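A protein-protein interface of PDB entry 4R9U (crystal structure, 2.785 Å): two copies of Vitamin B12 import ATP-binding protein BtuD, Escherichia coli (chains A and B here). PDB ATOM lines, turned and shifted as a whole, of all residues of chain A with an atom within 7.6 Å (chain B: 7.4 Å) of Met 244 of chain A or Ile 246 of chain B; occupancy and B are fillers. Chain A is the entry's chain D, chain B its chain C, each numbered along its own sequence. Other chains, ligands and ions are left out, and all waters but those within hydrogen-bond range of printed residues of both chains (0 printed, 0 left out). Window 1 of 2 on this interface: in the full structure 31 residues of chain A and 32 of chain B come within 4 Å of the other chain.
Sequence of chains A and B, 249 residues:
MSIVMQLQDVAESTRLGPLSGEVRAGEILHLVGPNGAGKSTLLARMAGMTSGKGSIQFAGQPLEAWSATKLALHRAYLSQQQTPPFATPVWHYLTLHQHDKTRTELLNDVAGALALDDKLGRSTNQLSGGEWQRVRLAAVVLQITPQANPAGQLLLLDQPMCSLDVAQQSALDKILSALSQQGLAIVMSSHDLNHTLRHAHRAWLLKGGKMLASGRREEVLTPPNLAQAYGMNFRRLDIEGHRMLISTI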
ATOM      1  N   LEU A 193       0.044   4.185  -4.516  1.00  0.00           N
ATOM      2  CA  LEU A 193       1.171   3.382  -4.037  1.00  0.00           C
ATOM      3  C   LEU A 193       0.741   2.201  -3.176  1.00  0.00           C
ATOM      4  O   LEU A 193       1.222   1.093  -3.387  1.00  0.00           O
ATOM      5  CB  LEU A 193       2.165   4.207  -3.241  1.00  0.00           C
ATOM      6  CG  LEU A 193       3.065   5.197  -3.960  1.00  0.00           C
ATOM      7  CD1 LEU A 193       3.055   5.117  -5.486  1.00  0.00           C
ATOM      8  CD2 LEU A 193       2.415   6.456  -3.507  1.00  0.00           C
ATOM      9  N   ASN A 194      -0.165   2.439  -2.226  1.00  0.00           N
ATOM     10  CA  ASN A 194      -0.585   1.403  -1.303  1.00  0.00           C
ATOM     11  C   ASN A 194      -1.131   0.212  -2.052  1.00  0.00           C
ATOM     12  O   ASN A 194      -0.760  -0.939  -1.793  1.00  0.00           O
ATOM     13  CB  ASN A 194      -1.622   1.979  -0.349  1.00  0.00           C
ATOM     14  CG  ASN A 194      -0.992   2.884   0.683  1.00  0.00           C
ATOM     15  OD1 ASN A 194      -0.095   2.486   1.421  1.00  0.00           O
ATOM     16  ND2 ASN A 194      -1.431   4.134   0.706  1.00  0.00           N
ATOM     17  N   LEU A 197       1.680  -1.738  -3.570  1.00  0.00           N
ATOM     18  CA  LEU A 197       2.333  -2.503  -2.511  1.00  0.00           C
ATOM     19  C   LEU A 197       1.561  -3.734  -2.109  1.00  0.00           C
ATOM     20  O   LEU A 197       2.150  -4.758  -1.762  1.00  0.00           O
ATOM     21  CB  LEU A 197       2.511  -1.651  -1.261  1.00  0.00           C
ATOM     22  CG  LEU A 197       3.900  -1.704  -0.664  1.00  0.00           C
ATOM     23  CD1 LEU A 197       4.730  -0.566  -1.195  1.00  0.00           C
ATOM     24  CD2 LEU A 197       3.708  -1.575   0.793  1.00  0.00           C
ATOM     25  N   ARG A 198       0.245  -3.642  -2.226  1.00  0.00           N
ATOM     26  CA  ARG A 198      -0.633  -4.718  -1.809  1.00  0.00           C
ATOM     27  C   ARG A 198      -0.920  -5.727  -2.925  1.00  0.00           C
ATOM     28  O   ARG A 198      -0.962  -6.924  -2.654  1.00  0.00           O
ATOM     29  CB  ARG A 198      -1.934  -4.141  -1.276  1.00  0.00           C
ATOM     30  CG  ARG A 198      -2.799  -5.197  -0.672  1.00  0.00           C
ATOM     31  CD  ARG A 198      -3.702  -4.661   0.415  1.00  0.00           C
ATOM     32  NE  ARG A 198      -4.808  -5.576   0.696  1.00  0.00           N
ATOM     33  CZ  ARG A 198      -5.664  -5.428   1.705  1.00  0.00           C
ATOM     34  NH1 ARG A 198      -5.526  -4.426   2.566  1.00  0.00           N
ATOM     35  NH2 ARG A 198      -6.635  -6.314   1.879  1.00  0.00           N
ATOM     36  N   ARG A 235       6.865   7.331   5.063  1.00  0.00           N
ATOM     37  CA  ARG A 235       7.094   6.330   6.067  1.00  0.00           C
ATOM     38  C   ARG A 235       6.357   5.027   5.710  1.00  0.00           C
ATOM     39  O   ARG A 235       5.249   5.053   5.186  1.00  0.00           O
ATOM     40  CB  ARG A 235       6.695   6.870   7.438  1.00  0.00           C
ATOM     41  CG  ARG A 235       7.668   6.399   8.513  1.00  0.00           C
ATOM     42  CD  ARG A 235       7.689   7.319   9.733  1.00  0.00           C
ATOM     43  NE  ARG A 235       6.481   7.062  10.502  1.00  0.00           N
ATOM     44  CZ  ARG A 235       6.129   7.693  11.614  1.00  0.00           C
ATOM     45  NH1 ARG A 235       5.000   7.399  12.247  1.00  0.00           N
ATOM     46  NH2 ARG A 235       6.916   8.635  12.095  1.00  0.00           N
ATOM     47  N   ARG A 236       7.037   3.899   5.901  1.00  0.00           N
ATOM     48  CA  ARG A 236       6.436   2.569   5.757  1.00  0.00           C
ATOM     49  C   ARG A 236       5.814   2.145   7.064  1.00  0.00           C
ATOM     50  O   ARG A 236       6.307   2.521   8.131  1.00  0.00           O
ATOM     51  CB  ARG A 236       7.481   1.534   5.379  1.00  0.00           C
ATOM     52  CG  ARG A 236       7.773   1.367   3.919  1.00  0.00           C
ATOM     53  CD  ARG A 236       6.853   0.317   3.319  1.00  0.00           C
ATOM     54  NE  ARG A 236       6.718  -0.853   4.185  1.00  0.00           N
ATOM     55  CZ  ARG A 236       6.543  -2.095   3.744  1.00  0.00           C
ATOM     56  NH1 ARG A 236       6.484  -2.352   2.445  1.00  0.00           N
ATOM     57  NH2 ARG A 236       6.440  -3.081   4.630  1.00  0.00           N
ATOM     58  N   LEU A 237       4.753   1.354   7.020  1.00  0.00           N
ATOM     59  CA  LEU A 237       4.199   0.837   8.256  1.00  0.00           C
ATOM     60  C   LEU A 237       3.438  -0.414   8.020  1.00  0.00           C
ATOM     61  O   LEU A 237       2.899  -0.623   6.941  1.00  0.00           O
ATOM     62  CB  LEU A 237       3.271   1.821   8.953  1.00  0.00           C
ATOM     63  CG  LEU A 237       3.115   3.211   8.451  1.00  0.00           C
ATOM     64  CD1 LEU A 237       1.632   3.274   8.376  1.00  0.00           C
ATOM     65  CD2 LEU A 237       3.685   4.097   9.510  1.00  0.00           C
ATOM     66  N   ASP A 238       3.386  -1.252   9.044  1.00  0.00           N
ATOM     67  CA  ASP A 238       2.845  -2.580   8.891  1.00  0.00           C
ATOM     68  C   ASP A 238       1.906  -2.850  10.071  1.00  0.00           C
ATOM     69  O   ASP A 238       2.347  -3.323  11.114  1.00  0.00           O
ATOM     70  CB  ASP A 238       3.960  -3.651   8.869  1.00  0.00           C
ATOM     71  CG  ASP A 238       5.032  -3.452   7.761  1.00  0.00           C
ATOM     72  OD1 ASP A 238       5.721  -4.474   7.493  1.00  0.00           O
ATOM     73  OD2 ASP A 238       5.218  -2.346   7.194  1.00  0.00           O
ATOM     74  N   ILE A 239       0.613  -2.587   9.917  1.00  0.00           N
ATOM     75  CA  ILE A 239      -0.300  -2.779  11.033  1.00  0.00           C
ATOM     76  C   ILE A 239      -1.268  -3.884  10.735  1.00  0.00           C
ATOM     77  O   ILE A 239      -1.849  -3.932   9.648  1.00  0.00           O
ATOM     78  CB  ILE A 239      -1.078  -1.510  11.377  1.00  0.00           C
ATOM     79  CG1 ILE A 239      -1.266  -0.625  10.137  1.00  0.00           C
ATOM     80  CG2 ILE A 239      -0.399  -0.789  12.530  1.00  0.00           C
ATOM     81  CD1 ILE A 239      -0.061   0.206   9.715  1.00  0.00           C
ATOM     82  N   GLU A 240      -1.390  -4.804  11.691  1.00  0.00           N
ATOM     83  CA  GLU A 240      -2.255  -5.962  11.557  1.00  0.00           C
ATOM     84  C   GLU A 240      -1.958  -6.738  10.294  1.00  0.00           C
ATOM     85  O   GLU A 240      -2.784  -7.541   9.854  1.00  0.00           O
ATOM     86  CB  GLU A 240      -3.719  -5.548  11.558  1.00  0.00           C
ATOM     87  CG  GLU A 240      -4.260  -5.299  12.930  1.00  0.00           C
ATOM     88  CD  GLU A 240      -5.534  -6.059  13.174  1.00  0.00           C
ATOM     89  OE1 GLU A 240      -5.748  -7.091  12.496  1.00  0.00           O
ATOM     90  OE2 GLU A 240      -6.322  -5.617  14.039  1.00  0.00           O
ATOM     91  N   GLY A 241      -0.809  -6.460   9.680  1.00  0.00           N
ATOM     92  CA  GLY A 241      -0.407  -7.125   8.460  1.00  0.00           C
ATOM     93  C   GLY A 241      -1.056  -6.487   7.250  1.00  0.00           C
ATOM     94  O   GLY A 241      -1.755  -7.145   6.466  1.00  0.00           O
ATOM     95  N   HIS A 242      -0.819  -5.192   7.090  1.00  0.00           N
ATOM     96  CA  HIS A 242      -1.380  -4.498   5.938  1.00  0.00           C
ATOM     97  C   HIS A 242      -0.411  -3.691   5.068  1.00  0.00           C
ATOM     98  O   HIS A 242      -0.749  -3.315   3.942  1.00  0.00           O
ATOM     99  CB  HIS A 242      -2.523  -3.620   6.387  1.00  0.00           C
ATOM    100  CG  HIS A 242      -3.810  -4.369   6.498  1.00  0.00           C
ATOM    101  ND1 HIS A 242      -4.298  -4.847   7.697  1.00  0.00           N
ATOM    102  CD2 HIS A 242      -4.682  -4.777   5.542  1.00  0.00           C
ATOM    103  CE1 HIS A 242      -5.435  -5.483   7.481  1.00  0.00           C
ATOM    104  NE2 HIS A 242      -5.689  -5.457   6.182  1.00  0.00           N
ATOM    105  N   ARG A 243       0.781  -3.428   5.591  1.00  0.00           N
ATOM    106  CA  ARG A 243       1.853  -2.724   4.871  1.00  0.00           C
ATOM    107  C   ARG A 243       1.422  -1.484   4.080  1.00  0.00           C
ATOM    108  O   ARG A 243       1.536  -1.440   2.873  1.00  0.00           O
ATOM    109  CB  ARG A 243       2.597  -3.739   3.965  1.00  0.00           C
ATOM    110  CG  ARG A 243       1.756  -4.462   2.921  1.00  0.00           C
ATOM    111  CD  ARG A 243       2.528  -5.527   2.148  1.00  0.00           C
ATOM    112  NE  ARG A 243       2.236  -6.849   2.710  1.00  0.00           N
ATOM    113  CZ  ARG A 243       3.095  -7.567   3.425  1.00  0.00           C
ATOM    114  NH1 ARG A 243       4.323  -7.109   3.604  1.00  0.00           N
ATOM    115  NH2 ARG A 243       2.754  -8.733   3.937  1.00  0.00           N
ATOM    116  N   MET A 244       0.891  -0.486   4.784  1.00  0.00           N
ATOM    117  CA  MET A 244       0.507   0.790   4.193  1.00  0.00           C
ATOM    118  C   MET A 244       1.696   1.759   4.018  1.00  0.00           C
ATOM    119  O   MET A 244       2.799   1.531   4.527  1.00  0.00           O
ATOM    120  CB  MET A 244      -0.563   1.460   5.040  1.00  0.00           C
ATOM    121  CG  MET A 244      -1.626   0.480   5.455  1.00  0.00           C
ATOM    122  SD  MET A 244      -2.811   1.166   6.624  1.00  0.00           S
ATOM    123  CE  MET A 244      -4.020   1.876   5.508  1.00  0.00           C
ATOM    124  N   LEU A 245       1.430   2.884   3.364  1.00  0.00           N
ATOM    125  CA  LEU A 245       2.454   3.877   3.053  1.00  0.00           C
ATOM    126  C   LEU A 245       1.998   5.297   3.332  1.00  0.00           C
ATOM    127  O   LEU A 245       1.188   5.839   2.617  1.00  0.00           O
ATOM    128  CB  LEU A 245       2.844   3.748   1.587  1.00  0.00           C
ATOM    129  CG  LEU A 245       4.290   3.304   1.420  1.00  0.00           C
ATOM    130  CD1 LEU A 245       4.596   2.971  -0.014  1.00  0.00           C
ATOM    131  CD2 LEU A 245       5.136   4.472   1.854  1.00  0.00           C
ATOM    132  N   ILE A 246       2.563   5.898   4.358  1.00  0.00           N
ATOM    133  CA  ILE A 246       2.140   7.227   4.785  1.00  0.00           C
ATOM    134  C   ILE A 246       3.097   8.298   4.278  1.00  0.00           C
ATOM    135  O   ILE A 246       4.260   8.003   4.026  1.00  0.00           O
ATOM    136  CB  ILE A 246       2.044   7.303   6.327  1.00  0.00           C
ATOM    137  CG1 ILE A 246       0.788   6.612   6.841  1.00  0.00           C
ATOM    138  CG2 ILE A 246       1.924   8.700   6.831  1.00  0.00           C
ATOM    139  CD1 ILE A 246       0.583   6.830   8.330  1.00  0.00           C
ATOM    140  N   ASN B 194      -9.583   7.425   2.920  1.00  0.00           N
ATOM    141  CA  ASN B 194      -8.490   7.884   3.774  1.00  0.00           C
ATOM    142  C   ASN B 194      -8.239   9.367   3.574  1.00  0.00           C
ATOM    143  O   ASN B 194      -8.099  10.138   4.528  1.00  0.00           O
ATOM    144  CB  ASN B 194      -7.217   7.090   3.479  1.00  0.00           C
ATOM    145  CG  ASN B 194      -7.257   5.705   4.085  1.00  0.00           C
ATOM    146  OD1 ASN B 194      -7.398   5.546   5.294  1.00  0.00           O
ATOM    147  ND2 ASN B 194      -7.161   4.690   3.241  1.00  0.00           N
ATOM    148  N   PRO B 223     -17.463   2.419   9.905  1.00  0.00           N
ATOM    149  CA  PRO B 223     -17.511   1.090   9.277  1.00  0.00           C
ATOM    150  C   PRO B 223     -18.916   0.531   8.933  1.00  0.00           C
ATOM    151  O   PRO B 223     -19.046  -0.044   7.852  1.00  0.00           O
ATOM    152  CB  PRO B 223     -16.792   0.209  10.303  1.00  0.00           C
ATOM    153  CG  PRO B 223     -15.784   1.137  10.917  1.00  0.00           C
ATOM    154  CD  PRO B 223     -16.408   2.514  10.926  1.00  0.00           C
ATOM    155  N   LEU B 226     -20.212   2.672   5.870  1.00  0.00           N
ATOM    156  CA  LEU B 226     -19.445   2.293   4.706  1.00  0.00           C
ATOM    157  C   LEU B 226     -19.862   0.905   4.274  1.00  0.00           C
ATOM    158  O   LEU B 226     -19.849   0.587   3.085  1.00  0.00           O
ATOM    159  CB  LEU B 226     -17.956   2.359   5.012  1.00  0.00           C
ATOM    160  CG  LEU B 226     -17.511   3.761   5.452  1.00  0.00           C
ATOM    161  CD1 LEU B 226     -16.068   3.767   5.939  1.00  0.00           C
ATOM    162  CD2 LEU B 226     -17.696   4.762   4.307  1.00  0.00           C
ATOM    163  N   MET B 232     -19.231  -3.810   2.196  1.00  0.00           N
ATOM    164  CA  MET B 232     -18.054  -4.542   2.655  1.00  0.00           C
ATOM    165  C   MET B 232     -17.556  -4.002   3.986  1.00  0.00           C
ATOM    166  O   MET B 232     -17.579  -2.794   4.228  1.00  0.00           O
ATOM    167  CB  MET B 232     -16.926  -4.500   1.609  1.00  0.00           C
ATOM    168  CG  MET B 232     -16.631  -3.132   1.040  1.00  0.00           C
ATOM    169  SD  MET B 232     -15.743  -3.211  -0.538  1.00  0.00           S
ATOM    170  CE  MET B 232     -14.116  -3.753  -0.027  1.00  0.00           C
ATOM    171  N   ASN B 233     -17.155  -4.915   4.862  1.00  0.00           N
ATOM    172  CA  ASN B 233     -16.584  -4.563   6.161  1.00  0.00           C
ATOM    173  C   ASN B 233     -15.350  -3.652   6.022  1.00  0.00           C
ATOM    174  O   ASN B 233     -14.607  -3.732   5.038  1.00  0.00           O
ATOM    175  CB  ASN B 233     -16.256  -5.839   6.942  1.00  0.00           C
ATOM    176  CG  ASN B 233     -17.416  -6.834   6.947  1.00  0.00           C
ATOM    177  OD1 ASN B 233     -18.563  -6.466   7.215  1.00  0.00           O
ATOM    178  ND2 ASN B 233     -17.122  -8.094   6.646  1.00  0.00           N
ATOM    179  N   PHE B 234     -15.134  -2.801   7.019  1.00  0.00           N
ATOM    180  CA  PHE B 234     -14.064  -1.823   6.989  1.00  0.00           C
ATOM    181  C   PHE B 234     -13.545  -1.627   8.407  1.00  0.00           C
ATOM    182  O   PHE B 234     -14.329  -1.392   9.312  1.00  0.00           O
ATOM    183  CB  PHE B 234     -14.584  -0.486   6.454  1.00  0.00           C
ATOM    184  CG  PHE B 234     -14.615  -0.384   4.965  1.00  0.00           C
ATOM    185  CD1 PHE B 234     -15.826  -0.218   4.303  1.00  0.00           C
ATOM    186  CD2 PHE B 234     -13.443  -0.435   4.220  1.00  0.00           C
ATOM    187  CE1 PHE B 234     -15.859  -0.123   2.922  1.00  0.00           C
ATOM    188  CE2 PHE B 234     -13.470  -0.342   2.834  1.00  0.00           C
ATOM    189  CZ  PHE B 234     -14.673  -0.188   2.185  1.00  0.00           C
ATOM    190  N   ARG B 235     -12.246  -1.736   8.625  1.00  0.00           N
ATOM    191  CA  ARG B 235     -11.738  -1.502   9.967  1.00  0.00           C
ATOM    192  C   ARG B 235     -11.000  -0.166  10.088  1.00  0.00           C
ATOM    193  O   ARG B 235     -10.283   0.248   9.179  1.00  0.00           O
ATOM    194  CB  ARG B 235     -10.846  -2.663  10.399  1.00  0.00           C
ATOM    195  CG  ARG B 235     -11.603  -3.977  10.581  1.00  0.00           C
ATOM    196  CD  ARG B 235     -10.698  -5.050  11.179  1.00  0.00           C
ATOM    197  NE  ARG B 235      -9.981  -4.566  12.361  1.00  0.00           N
ATOM    198  CZ  ARG B 235      -8.671  -4.331  12.400  1.00  0.00           C
ATOM    199  NH1 ARG B 235      -8.103  -3.889  13.516  1.00  0.00           N
ATOM    200  NH2 ARG B 235      -7.927  -4.541  11.321  1.00  0.00           N
ATOM    201  N   ARG B 236     -11.234   0.535  11.191  1.00  0.00           N
ATOM    202  CA  ARG B 236     -10.485   1.763  11.487  1.00  0.00           C
ATOM    203  C   ARG B 236      -9.188   1.488  12.211  1.00  0.00           C
ATOM    204  O   ARG B 236      -9.081   0.510  12.928  1.00  0.00           O
ATOM    205  CB  ARG B 236     -11.297   2.718  12.360  1.00  0.00           C
ATOM    206  CG  ARG B 236     -12.155   3.685  11.601  1.00  0.00           C
ATOM    207  CD  ARG B 236     -12.664   4.819  12.476  1.00  0.00           C
ATOM    208  NE  ARG B 236     -12.008   6.079  12.147  1.00  0.00           N
ATOM    209  CZ  ARG B 236     -12.630   7.252  12.121  1.00  0.00           C
ATOM    210  NH1 ARG B 236     -13.925   7.322  12.402  1.00  0.00           N
ATOM    211  NH2 ARG B 236     -11.956   8.352  11.815  1.00  0.00           N
ATOM    212  N   LEU B 237      -8.198   2.345  12.016  1.00  0.00           N
ATOM    213  CA  LEU B 237      -6.952   2.249  12.772  1.00  0.00           C
ATOM    214  C   LEU B 237      -6.277   3.594  12.786  1.00  0.00           C
ATOM    215  O   LEU B 237      -6.472   4.407  11.887  1.00  0.00           O
ATOM    216  CB  LEU B 237      -6.022   1.196  12.178  1.00  0.00           C
ATOM    217  CG  LEU B 237      -6.433   0.708  10.817  1.00  0.00           C
ATOM    218  CD1 LEU B 237      -5.383   1.199   9.867  1.00  0.00           C
ATOM    219  CD2 LEU B 237      -6.520  -0.790  10.870  1.00  0.00           C
ATOM    220  N   ILE B 239      -2.561   5.486  13.593  1.00  0.00           N
ATOM    221  CA  ILE B 239      -1.139   5.555  13.932  1.00  0.00           C
ATOM    222  C   ILE B 239      -0.508   6.924  13.845  1.00  0.00           C
ATOM    223  O   ILE B 239      -0.600   7.583  12.807  1.00  0.00           O
ATOM    224  CB  ILE B 239      -0.343   4.685  13.012  1.00  0.00           C
ATOM    225  CG1 ILE B 239      -0.999   3.323  12.956  1.00  0.00           C
ATOM    226  CG2 ILE B 239       1.093   4.591  13.475  1.00  0.00           C
ATOM    227  CD1 ILE B 239      -0.980   2.783  11.589  1.00  0.00           C
ATOM    228  N   ARG B 243      -5.305   8.100  11.500  1.00  0.00           N
ATOM    229  CA  ARG B 243      -6.654   7.481  11.405  1.00  0.00           C
ATOM    230  C   ARG B 243      -6.963   6.887  10.009  1.00  0.00           C
ATOM    231  O   ARG B 243      -7.894   7.308   9.331  1.00  0.00           O
ATOM    232  CB  ARG B 243      -7.763   8.460  11.813  1.00  0.00           C
ATOM    233  CG  ARG B 243      -7.909   9.690  10.948  1.00  0.00           C
ATOM    234  CD  ARG B 243      -8.944  10.589  11.500  1.00  0.00           C
ATOM    235  NE  ARG B 243      -8.398  11.700  12.258  1.00  0.00           N
ATOM    236  CZ  ARG B 243      -9.142  12.736  12.600  1.00  0.00           C
ATOM    237  NH1 ARG B 243     -10.419  12.766  12.235  1.00  0.00           N
ATOM    238  NH2 ARG B 243      -8.610  13.732  13.288  1.00  0.00           N
ATOM    239  N   MET B 244      -6.202   5.876   9.600  1.00  0.00           N
ATOM    240  CA  MET B 244      -6.365   5.285   8.279  1.00  0.00           C
ATOM    241  C   MET B 244      -7.641   4.421   8.190  1.00  0.00           C
ATOM    242  O   MET B 244      -8.359   4.262   9.182  1.00  0.00           O
ATOM    243  CB  MET B 244      -5.100   4.476   7.945  1.00  0.00           C
ATOM    244  CG  MET B 244      -3.806   5.281   8.197  1.00  0.00           C
ATOM    245  SD  MET B 244      -2.296   4.331   8.040  1.00  0.00           S
ATOM    246  CE  MET B 244      -1.953   4.610   6.305  1.00  0.00           C
ATOM    247  N   LEU B 245      -7.957   3.912   7.003  1.00  0.00           N
ATOM    248  CA  LEU B 245      -9.147   3.069   6.822  1.00  0.00           C
ATOM    249  C   LEU B 245      -8.881   1.833   5.993  1.00  0.00           C
ATOM    250  O   LEU B 245      -8.628   1.914   4.802  1.00  0.00           O
ATOM    251  CB  LEU B 245     -10.271   3.850   6.166  1.00  0.00           C
ATOM    252  CG  LEU B 245     -11.494   4.009   7.059  1.00  0.00           C
ATOM    253  CD1 LEU B 245     -12.489   4.917   6.386  1.00  0.00           C
ATOM    254  CD2 LEU B 245     -12.089   2.642   7.233  1.00  0.00           C
ATOM    255  N   ILE B 246      -8.936   0.681   6.632  1.00  0.00           N
ATOM    256  CA  ILE B 246      -8.615  -0.568   5.942  1.00  0.00           C
ATOM    257  C   ILE B 246      -9.861  -1.397   5.555  1.00  0.00           C
ATOM    258  O   ILE B 246     -10.874  -1.295   6.218  1.00  0.00           O
ATOM    259  CB  ILE B 246      -7.671  -1.391   6.822  1.00  0.00           C
ATOM    260  CG1 ILE B 246      -6.267  -0.787   6.821  1.00  0.00           C
ATOM    261  CG2 ILE B 246      -7.488  -2.791   6.326  1.00  0.00           C
ATOM    262  CD1 ILE B 246      -5.277  -1.641   7.625  1.00  0.00           C
ATOM    263  N   SER B 247      -9.766  -2.252   4.526  1.00  0.00           N
ATOM    264  CA  SER B 247     -10.884  -3.103   4.101  1.00  0.00           C
ATOM    265  C   SER B 247     -10.584  -4.568   4.358  1.00  0.00           C
ATOM    266  O   SER B 247      -9.466  -5.037   4.120  1.00  0.00           O
ATOM    267  CB  SER B 247     -11.177  -2.928   2.606  1.00  0.00           C
ATOM    268  OG  SER B 247     -10.068  -3.316   1.807  1.00  0.00           O
ATOM    269  N   THR B 248     -11.595  -5.290   4.828  1.00  0.00           N
ATOM    270  CA  THR B 248     -11.493  -6.727   4.985  1.00  0.00           C
ATOM    271  C   THR B 248     -12.183  -7.344   3.793  1.00  0.00           C
ATOM    272  O   THR B 248     -13.401  -7.543   3.792  1.00  0.00           O
ATOM    273  CB  THR B 248     -12.144  -7.228   6.278  1.00  0.00           C
ATOM    274  OG1 THR B 248     -11.563  -6.560   7.401  1.00  0.00           O
ATOM    275  CG2 THR B 248     -11.947  -8.730   6.410  1.00  0.00           C
ATOM    276  N   ILE B 249     -11.398  -7.644   2.766  1.00  0.00           N
ATOM    277  CA  ILE B 249     -11.943  -8.152   1.518  1.00  0.00           C
ATOM    278  C   ILE B 249     -12.069  -9.668   1.563  1.00  0.00           C
ATOM    279  O   ILE B 249     -11.450 -10.330   2.395  1.00  0.00           O
ATOM    280  CB  ILE B 249     -11.068  -7.744   0.315  1.00  0.00           C
ATOM    281  CG1 ILE B 249     -10.600  -6.295   0.464  1.00  0.00           C
ATOM    282  CG2 ILE B 249     -11.839  -7.910  -0.977  1.00  0.00           C
ATOM    283  CD1 ILE B 249      -9.474  -5.912  -0.475  1.00  0.00           C
ATOM    284  OXT ILE B 249     -12.805 -10.266   0.776  1.00  0.00           O
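Hydrophobic or aromatic side chains of chain A that line the printed part of chain B: Ile 239, His 242, Met 244 and Ile 246.
Of the 17 printed residues of chain B, 6 touch a printed residue of chain A.
Hydrophobic or aromatic side chains of chain B within 4 Å of the printed part of chain A: Ile 239, Met 244, Ile 246 and Ile 249.
NH2 of Arg 198 of chain A touches O of Ser 247 of chain B (3.8 Å).
Arg 198 of chain A touches Ile 249 of chain B.
Ile 239 of chain A touches Ile 239 of chain B (CD1 to CD1, 3.3 Å).
His 242 of chain A touches Ile 246 of chain B (NE2 to CG2, 3.2 Å).
Met 244 of chain A touches Ile 246 of chain B.
Met 244 of chain B touches Ile 246 of chain A (CE to CG1, 3.4 Å).
Of the printed residues of chain B, Glu 240 of chain A touches Arg 235 (2.5 Å).
Of chain B, only Met 244 and Ile 246 come within 4 Å of Met 244 of chain A.
Of chain A, only His 242 (3.2 Å) and Met 244 (3.7 Å) come within 4 Å of Ile 246 of chain B.
Printed residues of chain A within 4 Å of Ser 247 of chain B: Arg 198 (3.8 Å).
Thr 248 of chain B touches none of the printed residues of chain A.
Printed residues of chain A within 4 Å of Ile 249 of chain B: Arg 198 (3.7 Å).
The nearest residue of chain B that does not touch Met 244 of chain A is Leu 237 of chain B (4.1 Å).
The nearest residue of chain A that does not touch Ile 246 of chain B is Arg 198 of chain A (4.5 Å).
The guanidinium group of Arg 235 of chain B lies within salt-bridge range of the side-chain carboxylate of Glu 240 of chain A (2.5 Å).
The side-chain sulfur (SD) of Met 244 of chain A lies close to the side-chain sulfur (SD) of Met 244 of chain B (3.5 Å).
Ile 239 of chain B touches its own counterpart, Ile 239 of chain A.
Met 244 of chain B touches its own counterpart, Met 244 of chain A.
Met 244 of chain A touches Ile 246 of chain B, and with the chains exchanged Ile 246 of chain A touches Met 244 of chain B.
Of the 8 pairs that touch across the chains among the printed residues, 4 have their exchanged pair printed and touching as well.
O of Leu 237 of chain B is in hydrogen-bond range of N of Met 244 of chain B, 2.7 Å away.
N of Arg 235 of chain A sits at hydrogen-bond distance from O of Ile 246 of chain A (2.9 Å).
O of Ile 239 of chain A is in hydrogen-bond range of ND1 of His 242 of chain A.
O of Leu 237 of chain A lies within hydrogen-bond range of N of Met 244 of chain A, at 3.0 Å.
O of Ile 246 of chain B sits at hydrogen-bond distance from N of Arg 235 of chain B, at 2.8 Å.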
